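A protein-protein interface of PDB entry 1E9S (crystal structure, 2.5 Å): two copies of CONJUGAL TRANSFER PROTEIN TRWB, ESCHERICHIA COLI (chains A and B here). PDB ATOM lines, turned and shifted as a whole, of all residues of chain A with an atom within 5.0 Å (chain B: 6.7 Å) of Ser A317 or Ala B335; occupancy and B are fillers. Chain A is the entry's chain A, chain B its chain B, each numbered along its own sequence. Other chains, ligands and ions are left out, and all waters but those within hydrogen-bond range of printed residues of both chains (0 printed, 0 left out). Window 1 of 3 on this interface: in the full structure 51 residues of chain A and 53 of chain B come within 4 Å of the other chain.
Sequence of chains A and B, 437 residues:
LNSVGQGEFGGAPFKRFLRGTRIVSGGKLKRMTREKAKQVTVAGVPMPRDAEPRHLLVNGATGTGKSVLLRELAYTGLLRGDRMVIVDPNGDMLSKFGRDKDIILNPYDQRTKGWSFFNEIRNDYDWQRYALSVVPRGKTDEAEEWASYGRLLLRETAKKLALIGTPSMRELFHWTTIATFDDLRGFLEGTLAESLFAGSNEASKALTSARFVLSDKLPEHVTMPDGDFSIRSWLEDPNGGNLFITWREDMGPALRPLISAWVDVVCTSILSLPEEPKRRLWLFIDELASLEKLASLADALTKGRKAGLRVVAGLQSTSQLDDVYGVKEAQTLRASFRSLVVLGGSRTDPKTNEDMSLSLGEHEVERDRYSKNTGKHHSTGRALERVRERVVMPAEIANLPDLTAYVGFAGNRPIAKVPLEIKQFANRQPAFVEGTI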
ATOM      1  N   LEU A 315     -30.250 -13.682   4.759  1.00  0.00           N
ATOM      2  CA  LEU A 315     -29.084 -14.166   5.481  1.00  0.00           C
ATOM      3  C   LEU A 315     -28.978 -15.668   5.260  1.00  0.00           C
ATOM      4  O   LEU A 315     -29.963 -16.320   4.945  1.00  0.00           O
ATOM      5  CB  LEU A 315     -29.246 -13.861   6.971  1.00  0.00           C
ATOM      6  CG  LEU A 315     -28.373 -12.791   7.641  1.00  0.00           C
ATOM      7  CD1 LEU A 315     -28.161 -11.607   6.738  1.00  0.00           C
ATOM      8  CD2 LEU A 315     -29.043 -12.353   8.933  1.00  0.00           C
ATOM      9  N   GLN A 316     -27.784 -16.218   5.408  1.00  0.00           N
ATOM     10  CA  GLN A 316     -27.594 -17.650   5.230  1.00  0.00           C
ATOM     11  C   GLN A 316     -26.979 -18.243   6.488  1.00  0.00           C
ATOM     12  O   GLN A 316     -27.700 -18.731   7.350  1.00  0.00           O
ATOM     13  CB  GLN A 316     -26.716 -17.911   4.017  1.00  0.00           C
ATOM     14  CG  GLN A 316     -27.261 -17.232   2.772  1.00  0.00           C
ATOM     15  CD  GLN A 316     -26.476 -17.550   1.514  1.00  0.00           C
ATOM     16  OE1 GLN A 316     -26.399 -18.708   1.094  1.00  0.00           O
ATOM     17  NE2 GLN A 316     -25.890 -16.520   0.902  1.00  0.00           N
ATOM     18  N   SER A 317     -25.660 -18.195   6.613  1.00  0.00           N
ATOM     19  CA  SER A 317     -25.006 -18.720   7.809  1.00  0.00           C
ATOM     20  C   SER A 317     -24.786 -17.609   8.818  1.00  0.00           C
ATOM     21  O   SER A 317     -24.432 -16.490   8.461  1.00  0.00           O
ATOM     22  CB  SER A 317     -23.661 -19.357   7.467  1.00  0.00           C
ATOM     23  OG  SER A 317     -23.853 -20.529   6.698  1.00  0.00           O
ATOM     24  N   THR A 318     -25.008 -17.926  10.085  1.00  0.00           N
ATOM     25  CA  THR A 318     -24.831 -16.965  11.152  1.00  0.00           C
ATOM     26  C   THR A 318     -23.430 -16.378  11.083  1.00  0.00           C
ATOM     27  O   THR A 318     -23.242 -15.176  11.257  1.00  0.00           O
ATOM     28  CB  THR A 318     -25.051 -17.648  12.498  1.00  0.00           C
ATOM     29  OG1 THR A 318     -26.384 -18.172  12.526  1.00  0.00           O
ATOM     30  CG2 THR A 318     -24.864 -16.668  13.652  1.00  0.00           C
ATOM     31  N   SER A 319     -22.454 -17.235  10.798  1.00  0.00           N
ATOM     32  CA  SER A 319     -21.055 -16.845  10.708  1.00  0.00           C
ATOM     33  C   SER A 319     -20.740 -15.783   9.655  1.00  0.00           C
ATOM     34  O   SER A 319     -19.742 -15.078   9.764  1.00  0.00           O
ATOM     35  CB  SER A 319     -20.209 -18.085  10.453  1.00  0.00           C
ATOM     36  OG  SER A 319     -20.809 -18.898   9.468  1.00  0.00           O
ATOM     37  N   GLN A 320     -21.579 -15.671   8.635  1.00  0.00           N
ATOM     38  CA  GLN A 320     -21.372 -14.682   7.587  1.00  0.00           C
ATOM     39  C   GLN A 320     -21.486 -13.264   8.115  1.00  0.00           C
ATOM     40  O   GLN A 320     -20.572 -12.462   7.943  1.00  0.00           O
ATOM     41  CB  GLN A 320     -22.409 -14.847   6.502  1.00  0.00           C
ATOM     42  CG  GLN A 320     -22.005 -15.689   5.353  1.00  0.00           C
ATOM     43  CD  GLN A 320     -23.090 -15.713   4.308  1.00  0.00           C
ATOM     44  OE1 GLN A 320     -24.009 -16.532   4.360  1.00  0.00           O
ATOM     45  NE2 GLN A 320     -23.006 -14.793   3.363  1.00  0.00           N
ATOM     46  N   LEU A 321     -22.619 -12.952   8.739  1.00  0.00           N
ATOM     47  CA  LEU A 321     -22.832 -11.626   9.275  1.00  0.00           C
ATOM     48  C   LEU A 321     -21.878 -11.404  10.438  1.00  0.00           C
ATOM     49  O   LEU A 321     -21.390 -10.298  10.638  1.00  0.00           O
ATOM     50  CB  LEU A 321     -24.277 -11.474   9.740  1.00  0.00           C
ATOM     51  CG  LEU A 321     -24.729 -10.025   9.874  1.00  0.00           C
ATOM     52  CD1 LEU A 321     -24.718  -9.386   8.480  1.00  0.00           C
ATOM     53  CD2 LEU A 321     -26.102  -9.956  10.515  1.00  0.00           C
ATOM     54  N   SER A 346     -28.426 -26.273   5.258  1.00  0.00           N
ATOM     55  CA  SER A 346     -27.646 -27.461   4.972  1.00  0.00           C
ATOM     56  C   SER A 346     -27.394 -28.287   6.214  1.00  0.00           C
ATOM     57  O   SER A 346     -27.321 -27.753   7.312  1.00  0.00           O
ATOM     58  CB  SER A 346     -26.310 -27.054   4.351  1.00  0.00           C
ATOM     59  OG  SER A 346     -25.516 -28.192   4.064  1.00  0.00           O
ATOM     60  N   THR A 348     -24.767 -29.599   6.711  1.00  0.00           N
ATOM     61  CA  THR A 348     -23.361 -29.318   6.997  1.00  0.00           C
ATOM     62  C   THR A 348     -23.189 -28.029   7.809  1.00  0.00           C
ATOM     63  O   THR A 348     -22.065 -27.573   8.033  1.00  0.00           O
ATOM     64  CB  THR A 348     -22.554 -29.181   5.703  1.00  0.00           C
ATOM     65  OG1 THR A 348     -23.117 -28.121   4.929  1.00  0.00           O
ATOM     66  CG2 THR A 348     -22.581 -30.476   4.900  1.00  0.00           C
ATOM     67  N   ASP A 349     -24.301 -27.443   8.237  1.00  0.00           N
ATOM     68  CA  ASP A 349     -24.252 -26.228   9.036  1.00  0.00           C
ATOM     69  C   ASP A 349     -25.126 -26.396  10.276  1.00  0.00           C
ATOM     70  O   ASP A 349     -26.122 -25.690  10.458  1.00  0.00           O
ATOM     71  CB  ASP A 349     -24.736 -25.033   8.220  1.00  0.00           C
ATOM     72  CG  ASP A 349     -24.575 -23.718   8.950  1.00  0.00           C
ATOM     73  OD1 ASP A 349     -23.880 -23.672   9.991  1.00  0.00           O
ATOM     74  OD2 ASP A 349     -25.140 -22.715   8.470  1.00  0.00           O
ATOM     75  N   THR A 352     -25.959 -23.066  12.478  1.00  0.00           N
ATOM     76  CA  THR A 352     -26.992 -22.134  12.055  1.00  0.00           C
ATOM     77  C   THR A 352     -28.376 -22.744  12.227  1.00  0.00           C
ATOM     78  O   THR A 352     -29.346 -22.034  12.512  1.00  0.00           O
ATOM     79  CB  THR A 352     -26.798 -21.692  10.589  1.00  0.00           C
ATOM     80  OG1 THR A 352     -25.535 -21.024  10.449  1.00  0.00           O
ATOM     81  CG2 THR A 352     -27.895 -20.738  10.170  1.00  0.00           C
ATOM     82  N   LEU B  57     -20.025 -32.377  -0.147  1.00  0.00           N
ATOM     83  CA  LEU B  57     -18.902 -32.329   0.757  1.00  0.00           C
ATOM     84  C   LEU B  57     -18.690 -33.752   1.210  1.00  0.00           C
ATOM     85  O   LEU B  57     -19.617 -34.402   1.692  1.00  0.00           O
ATOM     86  CB  LEU B  57     -19.230 -31.433   1.955  1.00  0.00           C
ATOM     87  CG  LEU B  57     -18.203 -31.365   3.086  1.00  0.00           C
ATOM     88  CD1 LEU B  57     -16.865 -30.936   2.541  1.00  0.00           C
ATOM     89  CD2 LEU B  57     -18.685 -30.401   4.143  1.00  0.00           C
ATOM     90  N   LYS B 328     -15.185 -18.833  11.515  1.00  0.00           N
ATOM     91  CA  LYS B 328     -16.394 -18.202  10.959  1.00  0.00           C
ATOM     92  C   LYS B 328     -16.555 -18.443   9.454  1.00  0.00           C
ATOM     93  O   LYS B 328     -17.631 -18.814   9.000  1.00  0.00           O
ATOM     94  CB  LYS B 328     -16.383 -16.686  11.202  1.00  0.00           C
ATOM     95  CG  LYS B 328     -16.199 -16.216  12.649  1.00  0.00           C
ATOM     96  CD  LYS B 328     -17.510 -15.904  13.355  1.00  0.00           C
ATOM     97  CE  LYS B 328     -18.308 -17.179  13.656  1.00  0.00           C
ATOM     98  NZ  LYS B 328     -19.614 -16.936  14.370  1.00  0.00           N
ATOM     99  N   ALA B 330     -14.941 -20.727   7.731  1.00  0.00           N
ATOM    100  CA  ALA B 330     -14.910 -22.160   7.485  1.00  0.00           C
ATOM    101  C   ALA B 330     -16.329 -22.705   7.646  1.00  0.00           C
ATOM    102  O   ALA B 330     -16.733 -23.634   6.946  1.00  0.00           O
ATOM    103  CB  ALA B 330     -13.979 -22.843   8.459  1.00  0.00           C
ATOM    104  N   GLN B 331     -17.089 -22.134   8.575  1.00  0.00           N
ATOM    105  CA  GLN B 331     -18.464 -22.573   8.793  1.00  0.00           C
ATOM    106  C   GLN B 331     -19.354 -22.161   7.611  1.00  0.00           C
ATOM    107  O   GLN B 331     -20.225 -22.914   7.163  1.00  0.00           O
ATOM    108  CB  GLN B 331     -19.015 -21.957  10.073  1.00  0.00           C
ATOM    109  CG  GLN B 331     -20.390 -22.461  10.425  1.00  0.00           C
ATOM    110  CD  GLN B 331     -21.095 -21.565  11.411  1.00  0.00           C
ATOM    111  OE1 GLN B 331     -20.507 -21.136  12.412  1.00  0.00           O
ATOM    112  NE2 GLN B 331     -22.369 -21.280  11.144  1.00  0.00           N
ATOM    113  N   THR B 332     -19.135 -20.945   7.121  1.00  0.00           N
ATOM    114  CA  THR B 332     -19.892 -20.418   5.998  1.00  0.00           C
ATOM    115  C   THR B 332     -19.572 -21.274   4.769  1.00  0.00           C
ATOM    116  O   THR B 332     -20.465 -21.641   4.009  1.00  0.00           O
ATOM    117  CB  THR B 332     -19.515 -18.924   5.735  1.00  0.00           C
ATOM    118  OG1 THR B 332     -19.953 -18.115   6.838  1.00  0.00           O
ATOM    119  CG2 THR B 332     -20.154 -18.413   4.450  1.00  0.00           C
ATOM    120  N   LEU B 333     -18.297 -21.608   4.591  1.00  0.00           N
ATOM    121  CA  LEU B 333     -17.870 -22.417   3.456  1.00  0.00           C
ATOM    122  C   LEU B 333     -18.529 -23.792   3.520  1.00  0.00           C
ATOM    123  O   LEU B 333     -19.215 -24.194   2.589  1.00  0.00           O
ATOM    124  CB  LEU B 333     -16.340 -22.551   3.455  1.00  0.00           C
ATOM    125  CG  LEU B 333     -15.619 -22.888   2.146  1.00  0.00           C
ATOM    126  CD1 LEU B 333     -15.834 -21.780   1.127  1.00  0.00           C
ATOM    127  CD2 LEU B 333     -14.145 -23.051   2.420  1.00  0.00           C
ATOM    128  N   ARG B 334     -18.339 -24.505   4.625  1.00  0.00           N
ATOM    129  CA  ARG B 334     -18.928 -25.832   4.773  1.00  0.00           C
ATOM    130  C   ARG B 334     -20.437 -25.794   4.604  1.00  0.00           C
ATOM    131  O   ARG B 334     -21.013 -26.689   4.002  1.00  0.00           O
ATOM    132  CB  ARG B 334     -18.581 -26.444   6.136  1.00  0.00           C
ATOM    133  CG  ARG B 334     -17.183 -27.065   6.219  1.00  0.00           C
ATOM    134  CD  ARG B 334     -16.962 -27.753   7.562  1.00  0.00           C
ATOM    135  NE  ARG B 334     -17.017 -26.782   8.650  1.00  0.00           N
ATOM    136  CZ  ARG B 334     -15.961 -26.338   9.326  1.00  0.00           C
ATOM    137  NH1 ARG B 334     -14.741 -26.798   9.068  1.00  0.00           N
ATOM    138  NH2 ARG B 334     -16.133 -25.442  10.288  1.00  0.00           N
ATOM    139  N   ALA B 335     -21.076 -24.758   5.132  1.00  0.00           N
ATOM    140  CA  ALA B 335     -22.526 -24.621   5.021  1.00  0.00           C
ATOM    141  C   ALA B 335     -22.992 -24.445   3.579  1.00  0.00           C
ATOM    142  O   ALA B 335     -24.185 -24.513   3.309  1.00  0.00           O
ATOM    143  CB  ALA B 335     -23.003 -23.438   5.855  1.00  0.00           C
ATOM    144  N   SER B 336     -22.061 -24.223   2.655  1.00  0.00           N
ATOM    145  CA  SER B 336     -22.409 -24.012   1.246  1.00  0.00           C
ATOM    146  C   SER B 336     -22.571 -25.289   0.436  1.00  0.00           C
ATOM    147  O   SER B 336     -23.008 -25.238  -0.709  1.00  0.00           O
ATOM    148  CB  SER B 336     -21.363 -23.123   0.575  1.00  0.00           C
ATOM    149  OG  SER B 336     -21.299 -21.862   1.212  1.00  0.00           O
ATOM    150  N   PHE B 337     -22.183 -26.418   1.024  1.00  0.00           N
ATOM    151  CA  PHE B 337     -22.302 -27.726   0.388  1.00  0.00           C
ATOM    152  C   PHE B 337     -23.548 -28.348   0.995  1.00  0.00           C
ATOM    153  O   PHE B 337     -23.560 -28.692   2.171  1.00  0.00           O
ATOM    154  CB  PHE B 337     -21.085 -28.598   0.701  1.00  0.00           C
ATOM    155  CG  PHE B 337     -19.789 -28.084   0.118  1.00  0.00           C
ATOM    156  CD1 PHE B 337     -19.098 -27.044   0.724  1.00  0.00           C
ATOM    157  CD2 PHE B 337     -19.259 -28.656  -1.035  1.00  0.00           C
ATOM    158  CE1 PHE B 337     -17.900 -26.584   0.190  1.00  0.00           C
ATOM    159  CE2 PHE B 337     -18.061 -28.200  -1.573  1.00  0.00           C
ATOM    160  CZ  PHE B 337     -17.381 -27.160  -0.957  1.00  0.00           C
ATOM    161  N   ARG B 338     -24.596 -28.489   0.194  1.00  0.00           N
ATOM    162  CA  ARG B 338     -25.863 -29.018   0.679  1.00  0.00           C
ATOM    163  C   ARG B 338     -25.932 -30.531   0.897  1.00  0.00           C
ATOM    164  O   ARG B 338     -26.754 -31.011   1.687  1.00  0.00           O
ATOM    165  CB  ARG B 338     -26.979 -28.586  -0.269  1.00  0.00           C
ATOM    166  CG  ARG B 338     -27.188 -27.093  -0.339  1.00  0.00           C
ATOM    167  CD  ARG B 338     -27.736 -26.574   0.961  1.00  0.00           C
ATOM    168  NE  ARG B 338     -29.002 -27.220   1.316  1.00  0.00           N
ATOM    169  CZ  ARG B 338     -30.159 -26.994   0.707  1.00  0.00           C
ATOM    170  NH1 ARG B 338     -30.219 -26.129  -0.295  1.00  0.00           N
ATOM    171  NH2 ARG B 338     -31.257 -27.624   1.109  1.00  0.00           N
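Of the 11 printed residues of chain B, 8 touch a printed residue of chain A.
Printed residues of chain B that touch a printed residue of chain A: Leu B57, Lys B328, Gln B331, Thr B332, Arg B334, Ala B335, Phe B337 and Arg B338.
Along chain A the printed residues that touch a printed residue of chain B span positions 317 to 352.
Among the printed residues, 16 pairs touch across the chains.
Among the printed residues, no Asp or Glu carboxylate lies within 4 Å of a Lys or Arg side-chain nitrogen of the other chain.
No position is printed for both chains.
The side-chain hydroxyl (OG) of Ser A319 sits close to the backbone carbonyl oxygen (O) of Lys B328 (3.2 Å).
The side-chain hydroxyl of Ser A319 sits at hydrogen-bond distance from the side-chain amide nitrogen of Gln B331 (3.3 Å).
The side-chain hydroxyl (OG) of Ser A319 is in hydrogen-bond range of the side-chain hydroxyl (OG1) of Thr B332 (2.9 Å).
The backbone NH (N) of Gln A320 is in hydrogen-bond range of the side-chain hydroxyl (OG1) of Thr B332 (3.4 Å).
The side-chain hydroxyl (OG) of Ser A346 is in hydrogen-bond range of the backbone carbonyl oxygen (O) of Phe B337 (2.8 Å).
O of Arg B334 lies within hydrogen-bond range of OG1 of Thr A348.
OG1 of Thr A348 lies within hydrogen-bond range of O of Phe B337.
The side-chain carboxylate (OD1) of Asp A349 is in hydrogen-bond range of the side-chain amide nitrogen (NE2) of Gln B331 (3.1 Å).
The side-chain hydroxyl of Thr A352 is in hydrogen-bond range of the side-chain amide nitrogen of Gln B331 (3.3 Å).
The backbone NH (N) of Ser A317 is in hydrogen-bond range of the side-chain amide oxygen (OE1) of Gln A320 (3.3 Å).
The side-chain hydroxyl of Ser A317 sits at hydrogen-bond distance from the side-chain carboxylate of Asp A349, 3.1 Å away.
The side-chain hydroxyl (OG1) of Thr A352 lies within hydrogen-bond range of the backbone NH (N) of Thr A318 (3.2 Å).
The side-chain hydroxyl of Thr A348 lies within hydrogen-bond range of the side-chain hydroxyl of Ser A346.
OG1 of Thr A352 sits at hydrogen-bond distance from OD2 of Asp A349 (2.6 Å).
The side-chain hydroxyl (OG1) of Thr B332 sits at hydrogen-bond distance from the backbone carbonyl oxygen (O) of Lys B328, 3.2 Å away.
Ser A317 touches just these residues of chain B: Thr B332 and Ala B335.
Of the printed residues of chain B, Ser A346 touches Ala B335, Phe B337 and Arg B338.
Printed residues of chain B within 4 Å of Thr A348: Leu B57 (3.97 Å), Arg B334 (2.7 Å), Ala B335 (3.6 Å) and Phe B337 (2.9 Å).
Of the printed residues of chain A, Leu B57 touches Thr A348.
Of the printed residues of chain A, Lys B328 touches Ser A319.
Ala B330 touches none of the printed residues of chain A.
Of the printed residues of chain A, Gln B331 touches Ser A319, Asp A349 and Thr A352.
Of the printed residues of chain A, Ala B335 touches Ser A317, Ser A346, Thr A348 and Asp A349.
Ser B336 touches none of the printed residues of chain A.
The nearest printed residue of chain A that does not touch Gln B331 is Ser A317 (4.3 Å).
Among the printed residues, merely in contact across the chains: Ser A317 with Thr B332, Ser A317 with Ala B335, Ser A346 with Ala B335, Ser A346 with Arg B338, Thr A348 with Leu B57, Thr A348 with Ala B335 and Asp A349 with Ala B335.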
